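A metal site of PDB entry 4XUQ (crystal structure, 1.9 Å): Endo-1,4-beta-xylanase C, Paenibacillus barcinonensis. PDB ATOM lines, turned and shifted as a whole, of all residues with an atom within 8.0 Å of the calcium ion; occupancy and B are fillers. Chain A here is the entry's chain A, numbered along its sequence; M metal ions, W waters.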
ATOM      1  N   ALA A  18     -24.510   8.240 -24.370  1.00  0.00           N
ATOM      2  CA  ALA A  18     -23.963   6.906 -24.599  1.00  0.00           C
ATOM      3  C   ALA A  18     -24.986   6.077 -25.355  1.00  0.00           C
ATOM      4  O   ALA A  18     -26.014   5.721 -24.812  1.00  0.00           O
ATOM      5  CB  ALA A  18     -23.608   6.208 -23.275  1.00  0.00           C
ATOM      6  N   ASP A  19     -24.662   5.723 -26.581  1.00  0.00           N
ATOM      7  CA  ASP A  19     -25.522   4.826 -27.393  1.00  0.00           C
ATOM      8  C   ASP A  19     -24.872   3.451 -27.657  1.00  0.00           C
ATOM      9  O   ASP A  19     -25.522   2.569 -28.238  1.00  0.00           O
ATOM     10  CB  ASP A  19     -25.935   5.503 -28.661  1.00  0.00           C
ATOM     11  CG  ASP A  19     -24.741   5.816 -29.591  1.00  0.00           C
ATOM     12  OD1 ASP A  19     -23.664   5.223 -29.504  1.00  0.00           O
ATOM     13  OD2 ASP A  19     -24.916   6.705 -30.440  1.00  0.00           O
ATOM     14  N   PHE A  20     -23.605   3.289 -27.220  1.00  0.00           N
ATOM     15  CA  PHE A  20     -22.826   2.050 -27.326  1.00  0.00           C
ATOM     16  C   PHE A  20     -22.570   1.547 -28.749  1.00  0.00           C
ATOM     17  O   PHE A  20     -22.056   0.421 -28.958  1.00  0.00           O
ATOM     18  CB  PHE A  20     -23.503   0.978 -26.488  1.00  0.00           C
ATOM     19  CG  PHE A  20     -23.659   1.404 -25.076  1.00  0.00           C
ATOM     20  CD1 PHE A  20     -22.526   1.469 -24.225  1.00  0.00           C
ATOM     21  CD2 PHE A  20     -24.863   1.862 -24.614  1.00  0.00           C
ATOM     22  CE1 PHE A  20     -22.638   1.982 -22.940  1.00  0.00           C
ATOM     23  CE2 PHE A  20     -24.993   2.345 -23.302  1.00  0.00           C
ATOM     24  CZ  PHE A  20     -23.871   2.387 -22.490  1.00  0.00           C
ATOM     25  N   GLU A  21     -22.877   2.398 -29.728  1.00  0.00           N
ATOM     26  CA  GLU A  21     -22.833   1.969 -31.148  1.00  0.00           C
ATOM     27  C   GLU A  21     -21.398   1.762 -31.619  1.00  0.00           C
ATOM     28  O   GLU A  21     -21.160   0.989 -32.519  1.00  0.00           O
ATOM     29  CB  GLU A  21     -23.607   2.912 -32.032  1.00  0.00           C
ATOM     30  CG  GLU A  21     -25.129   2.840 -31.788  1.00  0.00           C
ATOM     31  CD  GLU A  21     -25.698   1.416 -31.821  1.00  0.00           C
ATOM     32  OE1 GLU A  21     -25.420   0.705 -32.786  1.00  0.00           O
ATOM     33  OE2 GLU A  21     -26.397   0.989 -30.878  1.00  0.00           O
ATOM     34  N   ASP A  22     -20.473   2.427 -30.974  1.00  0.00           N
ATOM     35  CA  ASP A  22     -19.027   2.198 -31.214  1.00  0.00           C
ATOM     36  C   ASP A  22     -18.504   0.903 -30.559  1.00  0.00           C
ATOM     37  O   ASP A  22     -17.367   0.530 -30.755  1.00  0.00           O
ATOM     38  CB  ASP A  22     -18.195   3.391 -30.752  1.00  0.00           C
ATOM     39  CG  ASP A  22     -18.363   3.720 -29.244  1.00  0.00           C
ATOM     40  OD1 ASP A  22     -19.034   2.960 -28.450  1.00  0.00           O
ATOM     41  OD2 ASP A  22     -17.867   4.796 -28.868  1.00  0.00           O
ATOM     42  N   VAL A  38     -20.757  -4.742 -23.585  1.00  0.00           N
ATOM     43  CA  VAL A  38     -21.449  -4.143 -24.722  1.00  0.00           C
ATOM     44  C   VAL A  38     -21.777  -5.292 -25.663  1.00  0.00           C
ATOM     45  O   VAL A  38     -20.878  -5.987 -26.167  1.00  0.00           O
ATOM     46  CB  VAL A  38     -20.632  -3.032 -25.425  1.00  0.00           C
ATOM     47  CG1 VAL A  38     -21.487  -2.380 -26.488  1.00  0.00           C
ATOM     48  CG2 VAL A  38     -20.228  -1.997 -24.401  1.00  0.00           C
ATOM     49  N   VAL A  39     -23.054  -5.495 -25.917  1.00  0.00           N
ATOM     50  CA  VAL A  39     -23.466  -6.597 -26.797  1.00  0.00           C
ATOM     51  C   VAL A  39     -23.879  -6.047 -28.142  1.00  0.00           C
ATOM     52  O   VAL A  39     -24.312  -4.891 -28.239  1.00  0.00           O
ATOM     53  CB  VAL A  39     -24.627  -7.425 -26.216  1.00  0.00           C
ATOM     54  CG1 VAL A  39     -24.218  -8.071 -24.904  1.00  0.00           C
ATOM     55  CG2 VAL A  39     -25.880  -6.573 -26.050  1.00  0.00           C
ATOM     56  N   ILE A  42     -28.670  -6.520 -29.939  1.00  0.00           N
ATOM     57  CA  ILE A  42     -29.699  -6.079 -28.998  1.00  0.00           C
ATOM     58  C   ILE A  42     -29.424  -4.587 -28.712  1.00  0.00           C
ATOM     59  O   ILE A  42     -28.335  -4.220 -28.339  1.00  0.00           O
ATOM     60  CB  ILE A  42     -29.650  -6.826 -27.635  1.00  0.00           C
ATOM     61  CG1 ILE A  42     -29.758  -8.361 -27.772  1.00  0.00           C
ATOM     62  CG2 ILE A  42     -30.741  -6.312 -26.686  1.00  0.00           C
ATOM     63  CD1 ILE A  42     -31.145  -8.848 -28.025  1.00  0.00           C
ATOM     64  N   GLY A  43     -30.458  -3.772 -28.885  1.00  0.00           N
ATOM     65  CA  GLY A  43     -30.343  -2.351 -28.609  1.00  0.00           C
ATOM     66  C   GLY A  43     -31.677  -1.677 -28.792  1.00  0.00           C
ATOM     67  O   GLY A  43     -32.602  -2.272 -29.341  1.00  0.00           O
ATOM     68  N   HIS A  44     -31.786  -0.445 -28.324  1.00  0.00           N
ATOM     69  CA  HIS A  44     -32.994   0.333 -28.482  1.00  0.00           C
ATOM     70  C   HIS A  44     -32.918   0.986 -29.859  1.00  0.00           C
ATOM     71  O   HIS A  44     -32.045   1.833 -30.064  1.00  0.00           O
ATOM     72  CB  HIS A  44     -33.113   1.418 -27.387  1.00  0.00           C
ATOM     73  CG  HIS A  44     -34.266   2.360 -27.594  1.00  0.00           C
ATOM     74  ND1 HIS A  44     -35.580   1.940 -27.695  1.00  0.00           N
ATOM     75  CD2 HIS A  44     -34.292   3.699 -27.758  1.00  0.00           C
ATOM     76  CE1 HIS A  44     -36.370   2.993 -27.862  1.00  0.00           C
ATOM     77  NE2 HIS A  44     -35.607   4.062 -27.882  1.00  0.00           N
ATOM     78  N   ASN A  45     -33.757   0.545 -30.794  1.00  0.00           N
ATOM     79  CA  ASN A  45     -33.668   1.009 -32.197  1.00  0.00           C
ATOM     80  C   ASN A  45     -32.263   1.091 -32.729  1.00  0.00           C
ATOM     81  O   ASN A  45     -31.869   2.088 -33.316  1.00  0.00           O
ATOM     82  CB  ASN A  45     -34.342   2.393 -32.298  1.00  0.00           C
ATOM     83  CG  ASN A  45     -35.818   2.344 -31.994  1.00  0.00           C
ATOM     84  OD1 ASN A  45     -36.376   3.286 -31.469  1.00  0.00           O
ATOM     85  ND2 ASN A  45     -36.464   1.211 -32.299  1.00  0.00           N
ATOM     86  N   SER A  46     -31.475   0.073 -32.444  1.00  0.00           N
ATOM     87  CA  SER A  46     -30.041   0.109 -32.717  1.00  0.00           C
ATOM     88  C   SER A  46     -29.498  -1.256 -32.461  1.00  0.00           C
ATOM     89  O   SER A  46     -30.198  -2.112 -31.945  1.00  0.00           O
ATOM     90  CB  SER A  46     -29.337   1.121 -31.819  1.00  0.00           C
ATOM     91  OG  SER A  46     -29.408   0.759 -30.445  1.00  0.00           O
ATOM     92  N   ASN A  47     -28.253  -1.445 -32.812  1.00  0.00           N
ATOM     93  CA  ASN A  47     -27.680  -2.740 -32.794  1.00  0.00           C
ATOM     94  C   ASN A  47     -26.876  -3.090 -31.547  1.00  0.00           C
ATOM     95  O   ASN A  47     -26.554  -4.259 -31.328  1.00  0.00           O
ATOM     96  CB  ASN A  47     -26.790  -2.896 -34.059  1.00  0.00           C
ATOM     97  CG  ASN A  47     -26.225  -4.299 -34.202  1.00  0.00           C
ATOM     98  OD1 ASN A  47     -25.000  -4.483 -34.272  1.00  0.00           O
ATOM     99  ND2 ASN A  47     -27.108  -5.299 -34.233  1.00  0.00           N
ATOM    100  N   ARG A  48     -26.530  -2.075 -30.734  1.00  0.00           N
ATOM    101  CA  ARG A  48     -25.733  -2.298 -29.549  1.00  0.00           C
ATOM    102  C   ARG A  48     -26.321  -1.650 -28.271  1.00  0.00           C
ATOM    103  O   ARG A  48     -26.956  -0.608 -28.346  1.00  0.00           O
ATOM    104  CB  ARG A  48     -24.303  -1.818 -29.733  1.00  0.00           C
ATOM    105  CG  ARG A  48     -23.654  -2.379 -30.994  1.00  0.00           C
ATOM    106  CD  ARG A  48     -22.263  -2.843 -30.746  1.00  0.00           C
ATOM    107  NE  ARG A  48     -21.467  -2.737 -31.949  1.00  0.00           N
ATOM    108  CZ  ARG A  48     -20.192  -3.104 -32.046  1.00  0.00           C
ATOM    109  NH1 ARG A  48     -19.565  -3.693 -31.031  1.00  0.00           N
ATOM    110  NH2 ARG A  48     -19.558  -2.897 -33.195  1.00  0.00           N
ATOM    111  N   SER A  49     -25.999  -2.260 -27.160  1.00  0.00           N
ATOM    112  CA  SER A  49     -26.396  -1.769 -25.851  1.00  0.00           C
ATOM    113  C   SER A  49     -25.529  -2.384 -24.769  1.00  0.00           C
ATOM    114  O   SER A  49     -24.690  -3.260 -25.064  1.00  0.00           O
ATOM    115  CB  SER A  49     -27.863  -2.038 -25.623  1.00  0.00           C
ATOM    116  OG  SER A  49     -28.117  -3.435 -25.636  1.00  0.00           O
ATOM    117  N   LEU A  50     -25.700  -1.911 -23.523  1.00  0.00           N
ATOM    118  CA  LEU A  50     -24.877  -2.322 -22.404  1.00  0.00           C
ATOM    119  C   LEU A  50     -25.657  -3.326 -21.607  1.00  0.00           C
ATOM    120  O   LEU A  50     -26.651  -2.980 -20.992  1.00  0.00           O
ATOM    121  CB  LEU A  50     -24.509  -1.111 -21.528  1.00  0.00           C
ATOM    122  CG  LEU A  50     -23.693  -1.409 -20.281  1.00  0.00           C
ATOM    123  CD1 LEU A  50     -22.391  -2.076 -20.675  1.00  0.00           C
ATOM    124  CD2 LEU A  50     -23.426  -0.126 -19.506  1.00  0.00           C
ATOM    125  N   TRP A 123     -38.580  -2.229 -24.400  1.00  0.00           N
ATOM    126  CA  TRP A 123     -37.746  -1.086 -24.037  1.00  0.00           C
ATOM    127  C   TRP A 123     -38.590   0.009 -23.482  1.00  0.00           C
ATOM    128  O   TRP A 123     -39.690   0.254 -23.960  1.00  0.00           O
ATOM    129  CB  TRP A 123     -36.976  -0.525 -25.247  1.00  0.00           C
ATOM    130  CG  TRP A 123     -35.868  -1.386 -25.675  1.00  0.00           C
ATOM    131  CD1 TRP A 123     -35.932  -2.375 -26.621  1.00  0.00           C
ATOM    132  CD2 TRP A 123     -34.511  -1.397 -25.171  1.00  0.00           C
ATOM    133  NE1 TRP A 123     -34.713  -3.007 -26.727  1.00  0.00           N
ATOM    134  CE2 TRP A 123     -33.809  -2.423 -25.877  1.00  0.00           C
ATOM    135  CE3 TRP A 123     -33.833  -0.675 -24.198  1.00  0.00           C
ATOM    136  CZ2 TRP A 123     -32.466  -2.739 -25.625  1.00  0.00           C
ATOM    137  CZ3 TRP A 123     -32.498  -0.950 -23.950  1.00  0.00           C
ATOM    138  CH2 TRP A 123     -31.807  -1.983 -24.677  1.00  0.00           C
ATOM    139  N   VAL A 166     -29.231  -1.554 -20.890  1.00  0.00           N
ATOM    140  CA  VAL A 166     -29.457  -0.131 -20.994  1.00  0.00           C
ATOM    141  C   VAL A 166     -28.877   0.436 -22.294  1.00  0.00           C
ATOM    142  O   VAL A 166     -27.938  -0.129 -22.843  1.00  0.00           O
ATOM    143  CB  VAL A 166     -28.900   0.664 -19.781  1.00  0.00           C
ATOM    144  CG1 VAL A 166     -29.510   0.151 -18.506  1.00  0.00           C
ATOM    145  CG2 VAL A 166     -27.390   0.601 -19.722  1.00  0.00           C
ATOM    146  N   ASP A 167     -29.437   1.543 -22.740  1.00  0.00           N
ATOM    147  CA  ASP A 167     -29.068   2.136 -24.003  1.00  0.00           C
ATOM    148  C   ASP A 167     -29.541   3.560 -24.028  1.00  0.00           C
ATOM    149  O   ASP A 167     -30.353   3.970 -23.231  1.00  0.00           O
ATOM    150  CB  ASP A 167     -29.715   1.338 -25.163  1.00  0.00           C
ATOM    151  CG  ASP A 167     -28.993   1.537 -26.492  1.00  0.00           C
ATOM    152  OD1 ASP A 167     -27.927   2.206 -26.537  1.00  0.00           O
ATOM    153  OD2 ASP A 167     -29.479   0.995 -27.509  1.00  0.00           O
ATOM    154  N   ASP A 168     -28.972   4.325 -24.945  1.00  0.00           N
ATOM    155  CA  ASP A 168     -29.439   5.692 -25.251  1.00  0.00           C
ATOM    156  C   ASP A 168     -29.472   6.569 -23.974  1.00  0.00           C
ATOM    157  O   ASP A 168     -30.492   7.153 -23.639  1.00  0.00           O
ATOM    158  CB  ASP A 168     -30.775   5.686 -25.941  1.00  0.00           C
ATOM    159  CG  ASP A 168     -30.669   5.265 -27.443  1.00  0.00           C
ATOM    160  OD1 ASP A 168     -29.561   5.202 -28.009  1.00  0.00           O
ATOM    161  OD2 ASP A 168     -31.721   4.978 -28.010  1.00  0.00           O
ATOM    162  N   VAL A 169     -28.353   6.564 -23.274  1.00  0.00           N
ATOM    163  CA  VAL A 169     -28.209   7.270 -22.003  1.00  0.00           C
ATOM    164  C   VAL A 169     -27.900   8.709 -22.405  1.00  0.00           C
ATOM    165  O   VAL A 169     -27.054   8.933 -23.285  1.00  0.00           O
ATOM    166  CB  VAL A 169     -27.085   6.670 -21.148  1.00  0.00           C
ATOM    167  CG1 VAL A 169     -26.952   7.438 -19.839  1.00  0.00           C
ATOM    168  CG2 VAL A 169     -27.340   5.211 -20.853  1.00  0.00           C
HETATM  169 CA    CA M   1     -27.536   1.508 -28.912  1.00  0.00          CA
HETATM  170  O   HOH W   1     -28.544   3.405 -29.627  1.00  0.00           O
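The backbone carbonyl oxygen (O) of His 44 sits close to the side-chain hydroxyl (OG) of Ser 46.
The backbone NH (N) of His 44 sits close to the side-chain carboxylate (OD2) of Asp 167.
The calcium ion is bound by water W1.
The calcium ion is bound by O of Arg 48 (2.3 Å).
The calcium ion is bound by the side-chain carboxylate (OE2) of Glu 21.
The calcium ion is bound by O of Asp 19.
OD2 of Asp 167 is bound to the calcium ion, at 2.5 Å.
The calcium ion is bound by OD1 of Asp 167 (2.5 Å).
OG of Ser 46 is bound to the calcium ion, at 2.5 Å.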
